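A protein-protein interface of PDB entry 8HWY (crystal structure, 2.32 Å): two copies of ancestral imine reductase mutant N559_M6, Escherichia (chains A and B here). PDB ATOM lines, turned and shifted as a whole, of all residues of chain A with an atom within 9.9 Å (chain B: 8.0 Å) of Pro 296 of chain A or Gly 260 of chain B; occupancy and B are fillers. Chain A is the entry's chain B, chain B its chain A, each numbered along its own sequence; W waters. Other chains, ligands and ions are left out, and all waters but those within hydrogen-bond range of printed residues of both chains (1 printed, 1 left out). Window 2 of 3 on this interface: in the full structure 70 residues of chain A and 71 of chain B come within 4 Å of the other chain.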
ATOM      1  N   ARG A 110      31.359  16.919 -17.580  1.00  0.00           N
ATOM      2  CA  ARG A 110      32.028  16.149 -16.540  1.00  0.00           C
ATOM      3  C   ARG A 110      33.359  15.586 -17.035  1.00  0.00           C
ATOM      4  O   ARG A 110      34.366  15.639 -16.316  1.00  0.00           O
ATOM      5  CB  ARG A 110      31.096  15.041 -16.070  1.00  0.00           C
ATOM      6  CG  ARG A 110      29.970  15.559 -15.199  1.00  0.00           C
ATOM      7  CD  ARG A 110      28.777  14.626 -15.195  1.00  0.00           C
ATOM      8  NE  ARG A 110      27.582  15.314 -14.724  1.00  0.00           N
ATOM      9  CZ  ARG A 110      26.366  15.013 -15.145  1.00  0.00           C
ATOM     10  NH1 ARG A 110      26.163  14.023 -15.997  1.00  0.00           N
ATOM     11  NH2 ARG A 110      25.328  15.711 -14.697  1.00  0.00           N
ATOM     12  N   LEU A 176      23.474  21.264 -18.534  1.00  0.00           N
ATOM     13  CA  LEU A 176      22.113  20.747 -18.530  1.00  0.00           C
ATOM     14  C   LEU A 176      21.142  21.892 -18.752  1.00  0.00           C
ATOM     15  O   LEU A 176      20.291  21.852 -19.654  1.00  0.00           O
ATOM     16  CB  LEU A 176      21.827  20.006 -17.220  1.00  0.00           C
ATOM     17  CG  LEU A 176      20.530  19.184 -17.200  1.00  0.00           C
ATOM     18  CD1 LEU A 176      20.604  17.989 -18.108  1.00  0.00           C
ATOM     19  CD2 LEU A 176      20.222  18.748 -15.809  1.00  0.00           C
ATOM     20  N   LEU A 272       2.940  12.082 -27.991  1.00  0.00           N
ATOM     21  CA  LEU A 272       3.230  12.335 -26.581  1.00  0.00           C
ATOM     22  C   LEU A 272       1.946  12.440 -25.766  1.00  0.00           C
ATOM     23  O   LEU A 272       1.824  11.858 -24.677  1.00  0.00           O
ATOM     24  CB  LEU A 272       4.043  13.624 -26.484  1.00  0.00           C
ATOM     25  CG  LEU A 272       4.826  13.953 -25.226  1.00  0.00           C
ATOM     26  CD1 LEU A 272       5.332  12.674 -24.529  1.00  0.00           C
ATOM     27  CD2 LEU A 272       5.977  14.864 -25.605  1.00  0.00           C
ATOM     28  N   ARG A 275       0.436   9.009 -25.327  1.00  0.00           N
ATOM     29  CA  ARG A 275       1.092   8.232 -24.275  1.00  0.00           C
ATOM     30  C   ARG A 275       0.540   8.614 -22.905  1.00  0.00           C
ATOM     31  O   ARG A 275       0.274   7.749 -22.066  1.00  0.00           O
ATOM     32  CB  ARG A 275       2.618   8.420 -24.313  1.00  0.00           C
ATOM     33  CG  ARG A 275       3.334   7.695 -25.511  1.00  0.00           C
ATOM     34  CD  ARG A 275       4.874   7.623 -25.326  1.00  0.00           C
ATOM     35  NE  ARG A 275       5.219   6.998 -24.054  1.00  0.00           N
ATOM     36  CZ  ARG A 275       6.076   7.500 -23.174  1.00  0.00           C
ATOM     37  NH1 ARG A 275       6.732   8.628 -23.416  1.00  0.00           N
ATOM     38  NH2 ARG A 275       6.284   6.856 -22.023  1.00  0.00           N
ATOM     39  N   VAL A 289       1.542  15.521 -19.085  1.00  0.00           N
ATOM     40  CA  VAL A 289       2.364  14.839 -20.077  1.00  0.00           C
ATOM     41  C   VAL A 289       3.803  14.682 -19.604  1.00  0.00           C
ATOM     42  O   VAL A 289       4.509  13.783 -20.067  1.00  0.00           O
ATOM     43  CB  VAL A 289       2.283  15.606 -21.413  1.00  0.00           C
ATOM     44  CG1 VAL A 289       3.464  15.294 -22.307  1.00  0.00           C
ATOM     45  CG2 VAL A 289       0.974  15.284 -22.105  1.00  0.00           C
ATOM     46  N   ILE A 290       4.266  15.540 -18.688  1.00  0.00           N
ATOM     47  CA  ILE A 290       5.625  15.413 -18.175  1.00  0.00           C
ATOM     48  C   ILE A 290       5.845  14.061 -17.518  1.00  0.00           C
ATOM     49  O   ILE A 290       6.975  13.561 -17.487  1.00  0.00           O
ATOM     50  CB  ILE A 290       5.954  16.556 -17.193  1.00  0.00           C
ATOM     51  CG1 ILE A 290       7.472  16.657 -17.002  1.00  0.00           C
ATOM     52  CG2 ILE A 290       5.233  16.350 -15.814  1.00  0.00           C
ATOM     53  CD1 ILE A 290       7.957  18.041 -16.626  1.00  0.00           C
ATOM     54  N   GLU A 291       4.776  13.432 -17.024  1.00  0.00           N
ATOM     55  CA  GLU A 291       4.911  12.132 -16.375  1.00  0.00           C
ATOM     56  C   GLU A 291       5.414  11.060 -17.337  1.00  0.00           C
ATOM     57  O   GLU A 291       6.092  10.120 -16.910  1.00  0.00           O
ATOM     58  CB  GLU A 291       3.570  11.725 -15.756  1.00  0.00           C
ATOM     59  CG  GLU A 291       3.198  12.608 -14.537  1.00  0.00           C
ATOM     60  CD  GLU A 291       4.221  12.496 -13.389  1.00  0.00           C
ATOM     61  OE1 GLU A 291       4.008  13.157 -12.335  1.00  0.00           O
ATOM     62  OE2 GLU A 291       5.231  11.747 -13.550  1.00  0.00           O
ATOM     63  N   VAL A 292       5.095  11.168 -18.630  1.00  0.00           N
ATOM     64  CA  VAL A 292       5.619  10.206 -19.594  1.00  0.00           C
ATOM     65  C   VAL A 292       6.923  10.663 -20.228  1.00  0.00           C
ATOM     66  O   VAL A 292       7.527   9.890 -20.983  1.00  0.00           O
ATOM     67  CB  VAL A 292       4.610   9.897 -20.719  1.00  0.00           C
ATOM     68  CG1 VAL A 292       3.353   9.326 -20.139  1.00  0.00           C
ATOM     69  CG2 VAL A 292       4.297  11.143 -21.544  1.00  0.00           C
ATOM     70  N   LEU A 293       7.352  11.907 -19.985  1.00  0.00           N
ATOM     71  CA  LEU A 293       8.645  12.370 -20.479  1.00  0.00           C
ATOM     72  C   LEU A 293       9.778  11.846 -19.614  1.00  0.00           C
ATOM     73  O   LEU A 293      10.850  11.500 -20.124  1.00  0.00           O
ATOM     74  CB  LEU A 293       8.684  13.895 -20.527  1.00  0.00           C
ATOM     75  CG  LEU A 293       7.650  14.467 -21.490  1.00  0.00           C
ATOM     76  CD1 LEU A 293       7.724  15.977 -21.526  1.00  0.00           C
ATOM     77  CD2 LEU A 293       7.828  13.873 -22.891  1.00  0.00           C
ATOM     78  N   ARG A 294       9.554  11.775 -18.304  1.00  0.00           N
ATOM     79  CA  ARG A 294      10.552  11.201 -17.413  1.00  0.00           C
ATOM     80  C   ARG A 294      10.754   9.724 -17.666  1.00  0.00           C
ATOM     81  O   ARG A 294      11.711   9.145 -17.144  1.00  0.00           O
ATOM     82  CB  ARG A 294      10.140  11.421 -15.966  1.00  0.00           C
ATOM     83  CG  ARG A 294       9.802  12.862 -15.668  1.00  0.00           C
ATOM     84  CD  ARG A 294       9.527  13.017 -14.211  1.00  0.00           C
ATOM     85  NE  ARG A 294       9.392  14.412 -13.852  1.00  0.00           N
ATOM     86  CZ  ARG A 294       8.324  14.881 -13.241  1.00  0.00           C
ATOM     87  NH1 ARG A 294       7.297  14.091 -12.961  1.00  0.00           N
ATOM     88  NH2 ARG A 294       8.302  16.156 -12.864  1.00  0.00           N
ATOM     89  N   LYS A 295       9.884   9.114 -18.458  1.00  0.00           N
ATOM     90  CA  LYS A 295       9.944   7.689 -18.745  1.00  0.00           C
ATOM     91  C   LYS A 295      10.371   7.474 -20.196  1.00  0.00           C
ATOM     92  O   LYS A 295       9.547   7.636 -21.110  1.00  0.00           O
ATOM     93  CB  LYS A 295       8.577   7.037 -18.475  1.00  0.00           C
ATOM     94  CG  LYS A 295       8.576   5.515 -18.634  1.00  0.00           C
ATOM     95  CD  LYS A 295       9.956   4.901 -18.231  1.00  0.00           C
ATOM     96  CE  LYS A 295      10.444   5.397 -16.871  1.00  0.00           C
ATOM     97  NZ  LYS A 295      11.923   5.364 -16.823  1.00  0.00           N
ATOM     98  N   PRO A 296      11.625   7.101 -20.468  1.00  0.00           N
ATOM     99  CA  PRO A 296      11.980   6.708 -21.840  1.00  0.00           C
ATOM    100  C   PRO A 296      10.983   5.686 -22.369  1.00  0.00           C
ATOM    101  O   PRO A 296      10.689   4.682 -21.708  1.00  0.00           O
ATOM    102  CB  PRO A 296      13.386   6.107 -21.696  1.00  0.00           C
ATOM    103  CG  PRO A 296      13.506   5.712 -20.261  1.00  0.00           C
ATOM    104  CD  PRO A 296      12.673   6.728 -19.498  1.00  0.00           C
ATOM    105  N   ALA A 297      10.452   5.956 -23.564  1.00  0.00           N
ATOM    106  CA  ALA A 297       9.421   5.114 -24.175  1.00  0.00           C
ATOM    107  C   ALA A 297      10.052   4.112 -25.139  1.00  0.00           C
ATOM    108  O   ALA A 297      11.199   4.285 -25.559  1.00  0.00           O
ATOM    109  CB  ALA A 297       8.368   5.980 -24.897  1.00  0.00           C
ATOM    110  N   ALA B 197      11.561  18.270 -17.874  1.00  0.00           N
ATOM    111  CA  ALA B 197      11.925  16.920 -17.498  1.00  0.00           C
ATOM    112  C   ALA B 197      13.431  16.748 -17.559  1.00  0.00           C
ATOM    113  O   ALA B 197      14.017  16.045 -16.724  1.00  0.00           O
ATOM    114  CB  ALA B 197      11.231  15.917 -18.405  1.00  0.00           C
ATOM    115  N   LEU B 198      14.061  17.363 -18.566  1.00  0.00           N
ATOM    116  CA  LEU B 198      15.511  17.308 -18.716  1.00  0.00           C
ATOM    117  C   LEU B 198      16.192  17.814 -17.457  1.00  0.00           C
ATOM    118  O   LEU B 198      16.980  17.107 -16.821  1.00  0.00           O
ATOM    119  CB  LEU B 198      15.944  18.138 -19.933  1.00  0.00           C
ATOM    120  CG  LEU B 198      17.240  17.771 -20.644  1.00  0.00           C
ATOM    121  CD1 LEU B 198      17.442  16.257 -20.654  1.00  0.00           C
ATOM    122  CD2 LEU B 198      17.181  18.313 -22.046  1.00  0.00           C
ATOM    123  N   SER B 201      15.606  15.862 -14.221  1.00  0.00           N
ATOM    124  CA  SER B 201      16.299  14.602 -14.003  1.00  0.00           C
ATOM    125  C   SER B 201      17.531  14.764 -13.126  1.00  0.00           C
ATOM    126  O   SER B 201      18.188  13.764 -12.815  1.00  0.00           O
ATOM    127  CB  SER B 201      16.685  14.000 -15.349  1.00  0.00           C
ATOM    128  OG  SER B 201      17.563  14.868 -16.049  1.00  0.00           O
ATOM    129  N   ILE B 253      19.424  15.514 -27.970  1.00  0.00           N
ATOM    130  CA  ILE B 253      19.062  14.099 -28.001  1.00  0.00           C
ATOM    131  C   ILE B 253      20.001  13.307 -27.109  1.00  0.00           C
ATOM    132  O   ILE B 253      19.558  12.575 -26.210  1.00  0.00           O
ATOM    133  CB  ILE B 253      19.060  13.565 -29.446  1.00  0.00           C
ATOM    134  CG1 ILE B 253      17.982  14.287 -30.245  1.00  0.00           C
ATOM    135  CG2 ILE B 253      18.806  12.028 -29.490  1.00  0.00           C
ATOM    136  CD1 ILE B 253      18.133  14.169 -31.729  1.00  0.00           C
ATOM    137  N   HIS B 254      21.314  13.480 -27.316  1.00  0.00           N
ATOM    138  CA  HIS B 254      22.311  12.794 -26.501  1.00  0.00           C
ATOM    139  C   HIS B 254      22.061  13.046 -25.034  1.00  0.00           C
ATOM    140  O   HIS B 254      21.980  12.103 -24.235  1.00  0.00           O
ATOM    141  CB  HIS B 254      23.726  13.245 -26.867  1.00  0.00           C
ATOM    142  CG  HIS B 254      24.123  12.862 -28.248  1.00  0.00           C
ATOM    143  ND1 HIS B 254      23.562  11.786 -28.901  1.00  0.00           N
ATOM    144  CD2 HIS B 254      24.979  13.434 -29.124  1.00  0.00           C
ATOM    145  CE1 HIS B 254      24.085  11.690 -30.110  1.00  0.00           C
ATOM    146  NE2 HIS B 254      24.947  12.679 -30.269  1.00  0.00           N
ATOM    147  N   ALA B 255      21.931  14.320 -24.658  1.00  0.00           N
ATOM    148  CA  ALA B 255      21.700  14.635 -23.256  1.00  0.00           C
ATOM    149  C   ALA B 255      20.452  13.929 -22.755  1.00  0.00           C
ATOM    150  O   ALA B 255      20.454  13.362 -21.658  1.00  0.00           O
ATOM    151  CB  ALA B 255      21.574  16.144 -23.046  1.00  0.00           C
ATOM    152  N   SER B 256      19.387  13.930 -23.563  1.00  0.00           N
ATOM    153  CA  SER B 256      18.123  13.337 -23.134  1.00  0.00           C
ATOM    154  C   SER B 256      18.282  11.857 -22.874  1.00  0.00           C
ATOM    155  O   SER B 256      17.808  11.345 -21.851  1.00  0.00           O
ATOM    156  CB  SER B 256      17.043  13.568 -24.179  1.00  0.00           C
ATOM    157  OG  SER B 256      16.771  14.946 -24.226  1.00  0.00           O
ATOM    158  N   ARG B 257      18.946  11.152 -23.803  1.00  0.00           N
ATOM    159  CA  ARG B 257      19.181   9.722 -23.631  1.00  0.00           C
ATOM    160  C   ARG B 257      19.955   9.479 -22.362  1.00  0.00           C
ATOM    161  O   ARG B 257      19.581   8.632 -21.544  1.00  0.00           O
ATOM    162  CB  ARG B 257      19.955   9.134 -24.813  1.00  0.00           C
ATOM    163  CG  ARG B 257      19.132   8.735 -25.997  1.00  0.00           C
ATOM    164  CD  ARG B 257      19.935   7.782 -26.883  1.00  0.00           C
ATOM    165  NE  ARG B 257      20.071   8.262 -28.258  1.00  0.00           N
ATOM    166  CZ  ARG B 257      19.074   8.344 -29.132  1.00  0.00           C
ATOM    167  NH1 ARG B 257      17.826   8.070 -28.783  1.00  0.00           N
ATOM    168  NH2 ARG B 257      19.339   8.698 -30.391  1.00  0.00           N
ATOM    169  N   ALA B 258      21.004  10.268 -22.148  1.00  0.00           N
ATOM    170  CA  ALA B 258      21.897   9.992 -21.037  1.00  0.00           C
ATOM    171  C   ALA B 258      21.292  10.373 -19.692  1.00  0.00           C
ATOM    172  O   ALA B 258      21.790   9.914 -18.659  1.00  0.00           O
ATOM    173  CB  ALA B 258      23.231  10.705 -21.245  1.00  0.00           C
ATOM    174  N   GLN B 259      20.234  11.183 -19.677  1.00  0.00           N
ATOM    175  CA  GLN B 259      19.545  11.542 -18.444  1.00  0.00           C
ATOM    176  C   GLN B 259      18.290  10.708 -18.195  1.00  0.00           C
ATOM    177  O   GLN B 259      17.596  10.945 -17.202  1.00  0.00           O
ATOM    178  CB  GLN B 259      19.159  13.027 -18.464  1.00  0.00           C
ATOM    179  CG  GLN B 259      20.313  14.011 -18.469  1.00  0.00           C
ATOM    180  CD  GLN B 259      21.091  14.031 -17.160  1.00  0.00           C
ATOM    181  OE1 GLN B 259      22.320  13.908 -17.161  1.00  0.00           O
ATOM    182  NE2 GLN B 259      20.387  14.220 -16.040  1.00  0.00           N
ATOM    183  N   GLY B 260      17.961   9.760 -19.071  1.00  0.00           N
ATOM    184  CA  GLY B 260      16.764   8.963 -18.892  1.00  0.00           C
ATOM    185  C   GLY B 260      15.502   9.523 -19.517  1.00  0.00           C
ATOM    186  O   GLY B 260      14.481   8.824 -19.551  1.00  0.00           O
ATOM    187  N   ILE B 261      15.543  10.743 -20.026  1.00  0.00           N
ATOM    188  CA  ILE B 261      14.350  11.415 -20.522  1.00  0.00           C
ATOM    189  C   ILE B 261      13.967  10.833 -21.869  1.00  0.00           C
ATOM    190  O   ILE B 261      14.821  10.395 -22.639  1.00  0.00           O
ATOM    191  CB  ILE B 261      14.599  12.932 -20.622  1.00  0.00           C
ATOM    192  CG1 ILE B 261      14.928  13.490 -19.244  1.00  0.00           C
ATOM    193  CG2 ILE B 261      13.411  13.658 -21.234  1.00  0.00           C
ATOM    194  CD1 ILE B 261      14.119  12.864 -18.102  1.00  0.00           C
ATOM    195  N   ASP B 262      12.674  10.823 -22.161  1.00  0.00           N
ATOM    196  CA  ASP B 262      12.232  10.435 -23.491  1.00  0.00           C
ATOM    197  C   ASP B 262      12.791  11.388 -24.545  1.00  0.00           C
ATOM    198  O   ASP B 262      13.006  12.575 -24.292  1.00  0.00           O
ATOM    199  CB  ASP B 262      10.713  10.431 -23.546  1.00  0.00           C
ATOM    200  CG  ASP B 262      10.178  10.041 -24.902  1.00  0.00           C
ATOM    201  OD1 ASP B 262      10.408   8.901 -25.351  1.00  0.00           O
ATOM    202  OD2 ASP B 262       9.493  10.872 -25.523  1.00  0.00           O
ATOM    203  N   THR B 263      12.999  10.868 -25.752  1.00  0.00           N
ATOM    204  CA  THR B 263      13.662  11.638 -26.792  1.00  0.00           C
ATOM    205  C   THR B 263      12.836  11.773 -28.063  1.00  0.00           C
ATOM    206  O   THR B 263      13.299  12.413 -29.018  1.00  0.00           O
ATOM    207  CB  THR B 263      15.031  11.019 -27.125  1.00  0.00           C
ATOM    208  OG1 THR B 263      14.842   9.777 -27.810  1.00  0.00           O
ATOM    209  CG2 THR B 263      15.860  10.771 -25.849  1.00  0.00           C
ATOM    210  N   ALA B 264      11.625  11.217 -28.102  1.00  0.00           N
ATOM    211  CA  ALA B 264      10.810  11.286 -29.317  1.00  0.00           C
ATOM    212  C   ALA B 264      10.676  12.721 -29.866  1.00  0.00           C
ATOM    213  O   ALA B 264      10.789  12.956 -31.078  1.00  0.00           O
ATOM    214  CB  ALA B 264       9.443  10.662 -29.017  1.00  0.00           C
HETATM  215  O   HOH W   1      12.541  14.297 -14.721  1.00  0.00           O
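The backbone carbonyl oxygen (O) of Leu 293 of chain A lies within hydrogen-bond range of the backbone NH (N) of Asp 262 of chain B, at 2.8 Å. The backbone NH (N) of Ala 297 of chain A is in hydrogen-bond range of the side-chain carboxylate (OD1) of Asp 262 of chain B (3.4 Å). The backbone nitrogen of Pro 296 of chain A sits close to the backbone carbonyl oxygen of Gly 260 of chain B.
The backbone carbonyl oxygen of Leu 198 of chain B sits at hydrogen-bond distance from the side-chain hydroxyl of Ser 201 of chain B. The backbone carbonyl oxygen (O) of Ser 256 of chain B sits at hydrogen-bond distance from the backbone NH (N) of Ile 261 of chain B. N of Ala 264 of chain B lies within hydrogen-bond range of OD2 of Asp 262 of chain B. The guanidinium group of Arg 275 of chain A sits at hydrogen-bond distance from the backbone carbonyl oxygen of Lys 295 of chain A (3.5 Å). OE2 of Glu 291 of chain A lies within salt-bridge range of NH1 of Arg 294 of chain A.
Among the printed residues, pairs that only touch across the chains: Leu 176 of chain A with Leu 198 of chain B (3.8 Å), Ile 290 of chain A with Ala 197 of chain B (3.8 Å), Leu 293 of chain A with Ala 197 of chain B (3.9 Å), Leu 293 of chain A with Ile 261 of chain B (3.5 Å), Arg 294 of chain A with Gly 260 of chain B (3.7 Å), Arg 294 of chain A with Ile 261 of chain B (3.995 Å) and Lys 295 of chain A with Asp 262 of chain B (3.9 Å).
Gly 260 of chain B touches just these residues of chain A: Arg 294 (3.7 Å) and Pro 296 (2.8 Å). Of chain B, only Asp 262 (3.4 Å) comes within 4 Å of Ala 297 of chain A. No residue of chain A comes within 4 Å of Ala 258 of chain B. Printed residues of chain B within 4 Å of Leu 293 of chain A: Ala 197, Ile 261 and Asp 262. Of the printed residues of chain B, Leu 176 of chain A touches Leu 198 (3.8 Å). Of the printed residues of chain A, Ala 197 of chain B touches Ile 290 (3.8 Å) and Leu 293 (3.9 Å). Printed residues of chain A within 4 Å of Asp 262 of chain B: Leu 293 (2.8 Å), Lys 295 (3.9 Å) and Ala 297 (3.4 Å). Of the printed residues of chain B, Arg 294 of chain A touches Gly 260 and Ile 261. Ser 256 of chain B touches none of the printed residues of chain A. Val 289 of chain A touches none of the printed residues of chain B. The nearest residue of chain B that does not touch Pro 296 of chain A is Asp 262 of chain B (4.1 Å).
Printed residues of chain B that touch a printed residue of chain A: Ala 197, Leu 198, Gly 260, Ile 261 and Asp 262. Hydrophobic or aromatic side chains of chain B within 4 Å of the printed part of chain A: Ala 197 and Ile 261. Of the 13 printed residues of chain A, 7 touch a printed residue of chain B. Hydrophobic or aromatic side chains of chain A within 4 Å of the printed part of chain B: Leu 176, Ile 290, Leu 293, Pro 296 and Ala 297. Among the printed residues, 10 pairs touch across the chains. Among the printed residues, no Asp or Glu carboxylate lies within 4 Å of a Lys or Arg side-chain nitrogen of the other chain.
No position is printed for both chains. Of the 10 pairs that touch across the chains among the printed residues, none has its exchanged pair printed and touching as well.
Water W1 lies within hydrogen-bond range of O of Ala 197 of chain B (3.0 Å), NE of Arg 294 of chain A (3.3 Å) and N of Ser 201 of chain B (3.5 Å).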
